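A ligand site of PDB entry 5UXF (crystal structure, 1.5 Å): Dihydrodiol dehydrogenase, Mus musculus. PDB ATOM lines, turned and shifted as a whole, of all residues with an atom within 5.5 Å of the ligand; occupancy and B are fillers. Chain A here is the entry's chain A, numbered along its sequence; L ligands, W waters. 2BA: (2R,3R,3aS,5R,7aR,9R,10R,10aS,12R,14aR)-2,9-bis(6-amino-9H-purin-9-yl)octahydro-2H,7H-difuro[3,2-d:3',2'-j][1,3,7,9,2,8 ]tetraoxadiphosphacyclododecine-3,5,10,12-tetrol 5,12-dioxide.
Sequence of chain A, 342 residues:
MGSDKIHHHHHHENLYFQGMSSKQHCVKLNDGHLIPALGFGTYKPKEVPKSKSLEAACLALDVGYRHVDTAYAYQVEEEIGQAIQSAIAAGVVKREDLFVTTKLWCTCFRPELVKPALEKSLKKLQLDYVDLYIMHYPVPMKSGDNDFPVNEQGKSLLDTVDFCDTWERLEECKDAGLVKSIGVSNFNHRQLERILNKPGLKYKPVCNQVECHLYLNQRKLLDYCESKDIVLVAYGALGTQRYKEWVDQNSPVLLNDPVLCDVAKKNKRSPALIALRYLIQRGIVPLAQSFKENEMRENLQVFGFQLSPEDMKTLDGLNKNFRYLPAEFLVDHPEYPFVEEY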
ATOM      1  N   TYR A  43     -27.809  -5.304   9.033  1.00  0.00           N
ATOM      2  CA  TYR A  43     -26.370  -5.538   9.003  1.00  0.00           C
ATOM      3  C   TYR A  43     -25.851  -5.732  10.432  1.00  0.00           C
ATOM      4  O   TYR A  43     -26.213  -4.976  11.337  1.00  0.00           O
ATOM      5  CB  TYR A  43     -25.629  -4.381   8.338  1.00  0.00           C
ATOM      6  CG  TYR A  43     -24.132  -4.494   8.535  1.00  0.00           C
ATOM      7  CD1 TYR A  43     -23.383  -5.374   7.759  1.00  0.00           C
ATOM      8  CD2 TYR A  43     -23.485  -3.775   9.521  1.00  0.00           C
ATOM      9  CE1 TYR A  43     -22.015  -5.499   7.964  1.00  0.00           C
ATOM     10  CE2 TYR A  43     -22.131  -3.901   9.730  1.00  0.00           C
ATOM     11  CZ  TYR A  43     -21.400  -4.754   8.956  1.00  0.00           C
ATOM     12  OH  TYR A  43     -20.048  -4.849   9.176  1.00  0.00           O
ATOM     13  N   PRO A  45     -22.562  -5.833  12.874  1.00  0.00           N
ATOM     14  CA  PRO A  45     -21.131  -5.632  13.062  1.00  0.00           C
ATOM     15  C   PRO A  45     -20.501  -6.825  13.764  1.00  0.00           C
ATOM     16  O   PRO A  45     -21.171  -7.579  14.472  1.00  0.00           O
ATOM     17  CB  PRO A  45     -21.051  -4.372  13.928  1.00  0.00           C
ATOM     18  CG  PRO A  45     -22.380  -3.688  13.740  1.00  0.00           C
ATOM     19  CD  PRO A  45     -23.356  -4.823  13.594  1.00  0.00           C
ATOM     20  N   TYR A  74     -24.786 -11.290   5.752  1.00  0.00           N
ATOM     21  CA  TYR A  74     -24.786 -10.797   7.123  1.00  0.00           C
ATOM     22  C   TYR A  74     -24.779 -11.943   8.137  1.00  0.00           C
ATOM     23  O   TYR A  74     -24.497 -11.721   9.317  1.00  0.00           O
ATOM     24  CB  TYR A  74     -26.013  -9.892   7.402  1.00  0.00           C
ATOM     25  CG  TYR A  74     -26.222  -8.681   6.496  1.00  0.00           C
ATOM     26  CD1 TYR A  74     -25.207  -8.203   5.653  1.00  0.00           C
ATOM     27  CD2 TYR A  74     -27.451  -7.995   6.486  1.00  0.00           C
ATOM     28  CE1 TYR A  74     -25.419  -7.087   4.835  1.00  0.00           C
ATOM     29  CE2 TYR A  74     -27.672  -6.879   5.686  1.00  0.00           C
ATOM     30  CZ  TYR A  74     -26.653  -6.431   4.845  1.00  0.00           C
ATOM     31  OH  TYR A  74     -26.857  -5.334   4.020  1.00  0.00           O
ATOM     32  N   HIS A 136     -26.207  -8.449  -4.507  1.00  0.00           N
ATOM     33  CA  HIS A 136     -25.584  -7.628  -3.476  1.00  0.00           C
ATOM     34  C   HIS A 136     -24.585  -6.632  -4.059  1.00  0.00           C
ATOM     35  O   HIS A 136     -24.383  -5.548  -3.493  1.00  0.00           O
ATOM     36  CB  HIS A 136     -24.921  -8.554  -2.456  1.00  0.00           C
ATOM     37  CG  HIS A 136     -24.810  -8.000  -1.081  1.00  0.00           C
ATOM     38  ND1 HIS A 136     -25.028  -8.769   0.043  1.00  0.00           N
ATOM     39  CD2 HIS A 136     -24.455  -6.766  -0.623  1.00  0.00           C
ATOM     40  CE1 HIS A 136     -24.839  -8.043   1.121  1.00  0.00           C
ATOM     41  NE2 HIS A 136     -24.497  -6.819   0.754  1.00  0.00           N
ATOM     42  N   TYR A 137     -23.938  -6.996  -5.158  1.00  0.00           N
ATOM     43  CA  TYR A 137     -22.925  -6.189  -5.838  1.00  0.00           C
ATOM     44  C   TYR A 137     -22.988  -6.570  -7.311  1.00  0.00           C
ATOM     45  O   TYR A 137     -23.614  -7.579  -7.663  1.00  0.00           O
ATOM     46  CB  TYR A 137     -21.523  -6.461  -5.274  1.00  0.00           C
ATOM     47  CG  TYR A 137     -21.249  -5.811  -3.957  1.00  0.00           C
ATOM     48  CD1 TYR A 137     -20.899  -4.469  -3.898  1.00  0.00           C
ATOM     49  CD2 TYR A 137     -21.315  -6.528  -2.773  1.00  0.00           C
ATOM     50  CE1 TYR A 137     -20.641  -3.842  -2.693  1.00  0.00           C
ATOM     51  CE2 TYR A 137     -21.050  -5.897  -1.541  1.00  0.00           C
ATOM     52  CZ  TYR A 137     -20.711  -4.560  -1.522  1.00  0.00           C
ATOM     53  OH  TYR A 137     -20.466  -3.885  -0.334  1.00  0.00           O
ATOM     54  N   TYR A 235     -28.599   2.438   2.341  1.00  0.00           N
ATOM     55  CA  TYR A 235     -27.984   1.970   3.579  1.00  0.00           C
ATOM     56  C   TYR A 235     -26.874   2.929   4.000  1.00  0.00           C
ATOM     57  O   TYR A 235     -26.470   3.824   3.251  1.00  0.00           O
ATOM     58  CB  TYR A 235     -27.448   0.538   3.465  1.00  0.00           C
ATOM     59  CG  TYR A 235     -26.279   0.322   2.538  1.00  0.00           C
ATOM     60  CD1 TYR A 235     -24.965   0.432   2.979  1.00  0.00           C
ATOM     61  CD2 TYR A 235     -26.490  -0.014   1.191  1.00  0.00           C
ATOM     62  CE1 TYR A 235     -23.896   0.213   2.111  1.00  0.00           C
ATOM     63  CE2 TYR A 235     -25.428  -0.222   0.331  1.00  0.00           C
ATOM     64  CZ  TYR A 235     -24.147  -0.107   0.788  1.00  0.00           C
ATOM     65  OH  TYR A 235     -23.086  -0.316  -0.072  1.00  0.00           O
ATOM     66  N   GLY A 236     -26.394   2.753   5.237  1.00  0.00           N
ATOM     67  CA  GLY A 236     -25.487   3.736   5.786  1.00  0.00           C
ATOM     68  C   GLY A 236     -26.109   5.114   5.910  1.00  0.00           C
ATOM     69  O   GLY A 236     -25.398   6.121   5.830  1.00  0.00           O
ATOM     70  N   ALA A 237     -27.433   5.160   6.125  1.00  0.00           N
ATOM     71  CA  ALA A 237     -28.196   6.400   6.011  1.00  0.00           C
ATOM     72  C   ALA A 237     -27.835   7.431   7.073  1.00  0.00           C
ATOM     73  O   ALA A 237     -28.158   8.613   6.901  1.00  0.00           O
ATOM     74  CB  ALA A 237     -29.683   6.090   6.099  1.00  0.00           C
ATOM     75  N   LEU A 238     -27.198   7.016   8.164  1.00  0.00           N
ATOM     76  CA  LEU A 238     -26.759   7.918   9.221  1.00  0.00           C
ATOM     77  C   LEU A 238     -25.252   8.078   9.245  1.00  0.00           C
ATOM     78  O   LEU A 238     -24.695   8.568  10.236  1.00  0.00           O
ATOM     79  CB  LEU A 238     -27.273   7.441  10.575  1.00  0.00           C
ATOM     80  CG  LEU A 238     -28.802   7.352  10.711  1.00  0.00           C
ATOM     81  CD1 LEU A 238     -29.205   6.951  12.126  1.00  0.00           C
ATOM     82  CD2 LEU A 238     -29.451   8.682  10.330  1.00  0.00           C
ATOM     83  N   GLY A 239     -24.567   7.672   8.178  1.00  0.00           N
ATOM     84  CA  GLY A 239     -23.127   7.821   8.096  1.00  0.00           C
ATOM     85  C   GLY A 239     -22.328   6.665   8.640  1.00  0.00           C
ATOM     86  O   GLY A 239     -21.112   6.828   8.835  1.00  0.00           O
ATOM     87  N   THR A 240     -22.962   5.513   8.896  1.00  0.00           N
ATOM     88  CA  THR A 240     -22.308   4.309   9.429  1.00  0.00           C
ATOM     89  C   THR A 240     -21.656   4.542  10.799  1.00  0.00           C
ATOM     90  O   THR A 240     -21.512   3.605  11.582  1.00  0.00           O
ATOM     91  CB  THR A 240     -21.241   3.736   8.476  1.00  0.00           C
ATOM     92  OG1 THR A 240     -20.116   4.608   8.438  1.00  0.00           O
ATOM     93  CG2 THR A 240     -21.805   3.569   7.088  1.00  0.00           C
ATOM     94  N   LEU A 255     -23.265  12.367  12.219  1.00  0.00           N
ATOM     95  CA  LEU A 255     -24.249  12.774  13.215  1.00  0.00           C
ATOM     96  C   LEU A 255     -23.778  13.932  14.088  1.00  0.00           C
ATOM     97  O   LEU A 255     -24.611  14.561  14.736  1.00  0.00           O
ATOM     98  CB  LEU A 255     -24.637  11.575  14.082  1.00  0.00           C
ATOM     99  CG  LEU A 255     -25.529  10.596  13.312  1.00  0.00           C
ATOM    100  CD1 LEU A 255     -25.834   9.346  14.132  1.00  0.00           C
ATOM    101  CD2 LEU A 255     -26.816  11.286  12.873  1.00  0.00           C
ATOM    102  N   SER A 270     -34.062  15.180  16.397  1.00  0.00           N
ATOM    103  CA  SER A 270     -32.680  14.757  16.550  1.00  0.00           C
ATOM    104  C   SER A 270     -31.925  14.831  15.220  1.00  0.00           C
ATOM    105  O   SER A 270     -32.522  14.776  14.144  1.00  0.00           O
ATOM    106  CB  SER A 270     -32.619  13.336  17.089  1.00  0.00           C
ATOM    107  OG  SER A 270     -33.062  12.419  16.109  1.00  0.00           O
ATOM    108  N   ALA A 272     -30.264  12.474  13.850  1.00  0.00           N
ATOM    109  CA  ALA A 272     -30.572  11.255  13.110  1.00  0.00           C
ATOM    110  C   ALA A 272     -31.877  11.394  12.336  1.00  0.00           C
ATOM    111  O   ALA A 272     -31.964  10.974  11.180  1.00  0.00           O
ATOM    112  CB  ALA A 272     -30.652  10.046  14.054  1.00  0.00           C
ATOM    113  N   LEU A 287     -32.916   2.616   4.905  1.00  0.00           N
ATOM    114  CA  LEU A 287     -32.877   1.523   5.880  1.00  0.00           C
ATOM    115  C   LEU A 287     -32.332   2.107   7.172  1.00  0.00           C
ATOM    116  O   LEU A 287     -31.168   2.525   7.229  1.00  0.00           O
ATOM    117  CB  LEU A 287     -32.008   0.372   5.381  1.00  0.00           C
ATOM    118  CG  LEU A 287     -32.430  -0.156   4.008  1.00  0.00           C
ATOM    119  CD1 LEU A 287     -31.470  -1.266   3.559  1.00  0.00           C
ATOM    120  CD2 LEU A 287     -33.866  -0.636   4.030  1.00  0.00           C
ATOM    121  N   ALA A 288     -33.182   2.204   8.180  1.00  0.00           N
ATOM    122  CA  ALA A 288     -32.748   2.697   9.480  1.00  0.00           C
ATOM    123  C   ALA A 288     -32.450   1.501  10.366  1.00  0.00           C
ATOM    124  O   ALA A 288     -33.240   0.558  10.415  1.00  0.00           O
ATOM    125  CB  ALA A 288     -33.827   3.587  10.112  1.00  0.00           C
ATOM    126  N   GLN A 289     -31.323   1.527  11.057  1.00  0.00           N
ATOM    127  CA  GLN A 289     -31.136   0.448  12.010  1.00  0.00           C
ATOM    128  C   GLN A 289     -30.446   0.914  13.278  1.00  0.00           C
ATOM    129  O   GLN A 289     -29.607   1.829  13.278  1.00  0.00           O
ATOM    130  CB  GLN A 289     -30.374  -0.751  11.407  1.00  0.00           C
ATOM    131  CG  GLN A 289     -28.914  -0.550  11.053  1.00  0.00           C
ATOM    132  CD  GLN A 289     -28.304  -1.859  10.560  1.00  0.00           C
ATOM    133  OE1 GLN A 289     -28.238  -2.112   9.352  1.00  0.00           O
ATOM    134  NE2 GLN A 289     -27.923  -2.720  11.495  1.00  0.00           N
ATOM    135  N   SER A 290     -30.864   0.299  14.363  1.00  0.00           N
ATOM    136  CA  SER A 290     -30.226   0.421  15.655  1.00  0.00           C
ATOM    137  C   SER A 290     -30.483  -0.878  16.387  1.00  0.00           C
ATOM    138  O   SER A 290     -31.436  -1.594  16.088  1.00  0.00           O
ATOM    139  CB  SER A 290     -30.769   1.615  16.456  1.00  0.00           C
ATOM    140  OG  SER A 290     -30.109   1.696  17.703  1.00  0.00           O
ATOM    141  N   PHE A 291     -29.607  -1.191  17.336  1.00  0.00           N
ATOM    142  CA  PHE A 291     -29.875  -2.261  18.270  1.00  0.00           C
ATOM    143  C   PHE A 291     -30.486  -1.742  19.560  1.00  0.00           C
ATOM    144  O   PHE A 291     -30.777  -2.533  20.462  1.00  0.00           O
ATOM    145  CB  PHE A 291     -28.596  -3.060  18.533  1.00  0.00           C
ATOM    146  CG  PHE A 291     -28.002  -3.690  17.300  1.00  0.00           C
ATOM    147  CD1 PHE A 291     -28.612  -4.798  16.705  1.00  0.00           C
ATOM    148  CD2 PHE A 291     -26.851  -3.178  16.702  1.00  0.00           C
ATOM    149  CE1 PHE A 291     -28.095  -5.364  15.544  1.00  0.00           C
ATOM    150  CE2 PHE A 291     -26.332  -3.754  15.542  1.00  0.00           C
ATOM    151  CZ  PHE A 291     -26.955  -4.842  14.963  1.00  0.00           C
ATOM    152  N   LYS A 292     -30.722  -0.431  19.642  1.00  0.00           N
ATOM    153  CA  LYS A 292     -31.318   0.194  20.817  1.00  0.00           C
ATOM    154  C   LYS A 292     -32.796   0.488  20.553  1.00  0.00           C
ATOM    155  O   LYS A 292     -33.121   1.216  19.613  1.00  0.00           O
ATOM    156  CB  LYS A 292     -30.570   1.481  21.193  1.00  0.00           C
ATOM    157  CG  LYS A 292     -29.070   1.293  21.458  1.00  0.00           C
ATOM    158  CD  LYS A 292     -28.401   2.607  21.838  1.00  0.00           C
ATOM    159  CE  LYS A 292     -26.937   2.373  22.231  1.00  0.00           C
ATOM    160  NZ  LYS A 292     -26.112   1.992  21.047  1.00  0.00           N
ATOM    161  N   GLU A 295     -33.962   4.099  19.920  1.00  0.00           N
ATOM    162  CA  GLU A 295     -33.608   4.653  18.617  1.00  0.00           C
ATOM    163  C   GLU A 295     -34.475   4.087  17.503  1.00  0.00           C
ATOM    164  O   GLU A 295     -34.893   4.823  16.602  1.00  0.00           O
ATOM    165  CB  GLU A 295     -32.120   4.438  18.341  1.00  0.00           C
ATOM    166  CG  GLU A 295     -31.241   5.237  19.294  1.00  0.00           C
ATOM    167  CD  GLU A 295     -29.764   4.961  19.171  1.00  0.00           C
ATOM    168  OE1 GLU A 295     -29.358   4.070  18.390  1.00  0.00           O
ATOM    169  OE2 GLU A 295     -28.992   5.658  19.871  1.00  0.00           O
ATOM    170  N   GLU A 298     -37.620   6.064  17.767  1.00  0.00           N
ATOM    171  CA  GLU A 298     -37.413   7.427  17.293  1.00  0.00           C
ATOM    172  C   GLU A 298     -37.391   7.487  15.781  1.00  0.00           C
ATOM    173  O   GLU A 298     -37.989   8.389  15.184  1.00  0.00           O
ATOM    174  CB  GLU A 298     -36.115   8.004  17.868  1.00  0.00           C
ATOM    175  CG  GLU A 298     -36.049   9.497  17.535  1.00  0.00           C
ATOM    176  CD  GLU A 298     -34.728  10.195  17.806  1.00  0.00           C
ATOM    177  OE1 GLU A 298     -33.655   9.563  17.823  1.00  0.00           O
ATOM    178  OE2 GLU A 298     -34.767  11.434  17.959  1.00  0.00           O
ATOM    179  N   ASN A 299     -36.739   6.519  15.133  1.00  0.00           N
ATOM    180  CA  ASN A 299     -36.593   6.586  13.689  1.00  0.00           C
ATOM    181  C   ASN A 299     -37.941   6.479  12.990  1.00  0.00           C
ATOM    182  O   ASN A 299     -38.123   7.068  11.909  1.00  0.00           O
ATOM    183  CB  ASN A 299     -35.631   5.494  13.207  1.00  0.00           C
ATOM    184  CG  ASN A 299     -34.223   5.727  13.701  1.00  0.00           C
ATOM    185  OD1 ASN A 299     -33.876   6.834  14.119  1.00  0.00           O
ATOM    186  ND2 ASN A 299     -33.379   4.691  13.645  1.00  0.00           N
ATOM    187  N   LEU A 325     -18.239   3.075   2.861  1.00  0.00           N
ATOM    188  CA  LEU A 325     -18.293   1.636   2.597  1.00  0.00           C
ATOM    189  C   LEU A 325     -17.894   1.360   1.149  1.00  0.00           C
ATOM    190  O   LEU A 325     -18.729   1.027   0.305  1.00  0.00           O
ATOM    191  CB  LEU A 325     -19.684   1.086   2.905  1.00  0.00           C
ATOM    192  CG  LEU A 325     -20.092   1.281   4.382  1.00  0.00           C
ATOM    193  CD1 LEU A 325     -21.552   0.918   4.632  1.00  0.00           C
ATOM    194  CD2 LEU A 325     -19.166   0.453   5.283  1.00  0.00           C
HETATM  195  P   2BA L   1     -25.407   0.336  14.093  1.00  0.00           P
HETATM  196  O1P 2BA L   1     -26.611   0.152  14.950  1.00  0.00           O
HETATM  197  O2P 2BA L   1     -24.129  -0.394  14.436  1.00  0.00           O
HETATM  198  O5' 2BA L   1     -25.851  -0.024  12.585  1.00  0.00           O
HETATM  199  C5' 2BA L   1     -24.911  -0.576  11.665  1.00  0.00           C
HETATM  200  C4' 2BA L   1     -24.442   0.517  10.694  1.00  0.00           C
HETATM  201  O4' 2BA L   1     -23.394  -0.048   9.878  1.00  0.00           O
HETATM  202  C3' 2BA L   1     -25.505   1.010   9.736  1.00  0.00           C
HETATM  203  O3' 2BA L   1     -25.233   2.387   9.412  1.00  0.00           O
HETATM  204  C2' 2BA L   1     -25.215   0.172   8.506  1.00  0.00           C
HETATM  205  O2' 2BA L   1     -25.833   0.747   7.336  1.00  0.00           O
HETATM  206  C1' 2BA L   1     -23.696   0.199   8.500  1.00  0.00           C
HETATM  207  N9  2BA L   1     -22.957  -0.825   7.716  1.00  0.00           N
HETATM  208  C8  2BA L   1     -21.652  -1.127   7.897  1.00  0.00           C
HETATM  209  N7  2BA L   1     -21.238  -2.075   7.018  1.00  0.00           N
HETATM  210  C5  2BA L   1     -22.308  -2.373   6.251  1.00  0.00           C
HETATM  211  C6  2BA L   1     -22.566  -3.289   5.122  1.00  0.00           C
HETATM  212  N6  2BA L   1     -21.571  -4.089   4.650  1.00  0.00           N
HETATM  213  N1  2BA L   1     -23.804  -3.302   4.587  1.00  0.00           N
HETATM  214  C2  2BA L   1     -24.781  -2.520   5.056  1.00  0.00           C
HETATM  215  N3  2BA L   1     -24.620  -1.659   6.087  1.00  0.00           N
HETATM  216  C4  2BA L   1     -23.427  -1.536   6.701  1.00  0.00           C
HETATM  217  P1  2BA L   1     -26.325   3.572   9.585  1.00  0.00           P
HETATM  218 O1P1 2BA L   1     -25.688   4.787   8.978  1.00  0.00           O
HETATM  219 O2P1 2BA L   1     -27.662   3.068   9.115  1.00  0.00           O
HETATM  220 O5'1 2BA L   1     -26.460   3.774  11.175  1.00  0.00           O
HETATM  221 C5'1 2BA L   1     -25.283   4.146  11.864  1.00  0.00           C
HETATM  222 C4'1 2BA L   1     -25.542   4.145  13.362  1.00  0.00           C
HETATM  223 O4'1 2BA L   1     -26.545   5.106  13.717  1.00  0.00           O
HETATM  224 C3'1 2BA L   1     -26.114   2.854  13.900  1.00  0.00           C
HETATM  225 O3'1 2BA L   1     -25.062   1.901  14.027  1.00  0.00           O
HETATM  226 C2'1 2BA L   1     -26.721   3.295  15.215  1.00  0.00           C
HETATM  227 O2'1 2BA L   1     -25.772   3.095  16.262  1.00  0.00           O
HETATM  228 C1'1 2BA L   1     -26.940   4.781  15.046  1.00  0.00           C
HETATM  229  N91 2BA L   1     -28.341   5.214  15.179  1.00  0.00           N
HETATM  230  C81 2BA L   1     -29.424   4.654  14.584  1.00  0.00           C
HETATM  231  N71 2BA L   1     -30.543   5.337  14.907  1.00  0.00           N
HETATM  232  C51 2BA L   1     -30.176   6.347  15.711  1.00  0.00           C
HETATM  233  C61 2BA L   1     -30.869   7.434  16.406  1.00  0.00           C
HETATM  234  N61 2BA L   1     -32.203   7.583  16.299  1.00  0.00           N
HETATM  235  N11 2BA L   1     -30.121   8.284  17.152  1.00  0.00           N
HETATM  236  C21 2BA L   1     -28.783   8.134  17.251  1.00  0.00           C
HETATM  237  N31 2BA L   1     -28.071   7.161  16.646  1.00  0.00           N
HETATM  238  C41 2BA L   1     -28.728   6.264  15.880  1.00  0.00           C
HETATM  239  O   HOH W   1     -29.793   3.906  10.631  1.00  0.00           O
HETATM  240  O   HOH W   2     -21.817  -0.218  13.189  1.00  0.00           O
HETATM  241  O   HOH W   3     -28.756   2.107   6.939  1.00  0.00           O
HETATM  242  O   HOH W   4     -25.389   7.501  17.400  1.00  0.00           O
HETATM  243  O   HOH W   5     -31.061  10.513  18.252  1.00  0.00           O
HETATM  244  O   HOH W   6     -27.101   0.255  17.553  1.00  0.00           O
HETATM  245  O   HOH W   7     -23.349  -1.406  16.724  1.00  0.00           O
HETATM  246  O   HOH W   8     -28.470  -1.809  14.145  1.00  0.00           O
HETATM  247  O   HOH W   9     -18.809  -3.691   5.915  1.00  0.00           O
HETATM  248  O   HOH W  10     -28.817  -0.645   7.316  1.00  0.00           O
HETATM  249  O   HOH W  11     -24.934  -4.506   2.388  1.00  0.00           O
HETATM  250  O   HOH W  12     -26.939   2.809  18.606  1.00  0.00           O
HETATM  251  O   HOH W  13     -22.727   4.042  16.185  1.00  0.00           O
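The backbone carbonyl oxygen (O) of Glu 295 sits close to the side-chain amide nitrogen (ND2) of Asn 299 (3.3 Å). The side-chain hydroxyl (OG) of Ser 290 lies within hydrogen-bond range of the backbone NH (N) of Lys 292. OG of Ser 290 is in hydrogen-bond range of OE1 of Glu 295 (2.6 Å). The side-chain hydroxyl of Ser 270 lies within hydrogen-bond range of the side-chain carboxylate of Glu 298 (2.7 Å). NE2 of Gln 289 is in hydrogen-bond range of O of Tyr 43, 2.8 Å away.
Tyr 43 touches the ligand. Pro 45 touches the ligand. Tyr 74 touches the ligand (OH to C2, 3.6 Å). Tyr 235 touches the ligand (CD1 to C2, 3.6 Å). CB of Ala 272 touches C61 of the ligand, 3.5 Å away. O of Gln 289 touches C81 of the ligand, 3.1 Å away. Ser 290 touches the ligand (CA to O1P, 3.7 Å). CD2 of Phe 291 touches O1P of the ligand, 3.8 Å away. Glu 295 touches the ligand (OE1 to C41, 3.4 Å). CD2 of Leu 325 touches N7 of the ligand, 3.7 Å away. The nearest printed residue that does not touch the ligand is Leu 255 (4.01 Å).
The side-chain amide oxygen (OD1) of Asn 299 lies within hydrogen-bond range of a nitrogen (N61) of the ligand. The side-chain carboxylate (OE1) of Glu 298 lies within hydrogen-bond range of a nitrogen (N61) of the ligand, 2.9 Å away. The backbone NH (N) of Thr 240 is in hydrogen-bond range of an oxygen (O1P1) of the ligand (2.8 Å). The backbone NH (N) of Ala 237 lies within hydrogen-bond range of an oxygen (O1P1) of the ligand (3.4 Å). An oxygen (O1P1) of the ligand lies within hydrogen-bond range of the backbone NH (N) of Gly 239 (3.2 Å). The backbone NH (N) of Gly 236 is in hydrogen-bond range of an oxygen (O2') of the ligand, 3.0 Å away. N of Leu 238 lies within hydrogen-bond range of O1P1 of the ligand, 2.8 Å away.
Water W3 lies within hydrogen-bond range of the backbone carbonyl oxygen (O) of Leu 287 (2.5 Å), an oxygen (O2P1) of the ligand (2.6 Å), the backbone NH (N) of Gly 236 (3.0 Å) and the backbone NH (N) of Ala 237 (3.4 Å). Water W6 lies within hydrogen-bond range of an oxygen (O1P) of the ligand (2.7 Å), the backbone NH (N) of Phe 291 (2.9 Å) and the side-chain hydroxyl (OG) of Ser 290 (3.3 Å). Water W5 lies within hydrogen-bond range of N11 of the ligand (2.7 Å), OE1 of Glu 298 (2.8 Å) and OG of Ser 270 (3.5 Å). Water W1 bridges O2P1 of the ligand (2.7 Å) and N of Gln 289 (2.9 Å). Water W11 lies within hydrogen-bond range of the side-chain hydroxyl (OH) of Tyr 74 (2.7 Å), a nitrogen (N1) of the ligand (2.7 Å) and a ring nitrogen (NE2) of His 136 (2.9 Å). Water W10 bridges the side-chain amide oxygen (OE1) of Gln 289 (2.6 Å) and an oxygen (O2') of the ligand (3.3 Å).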
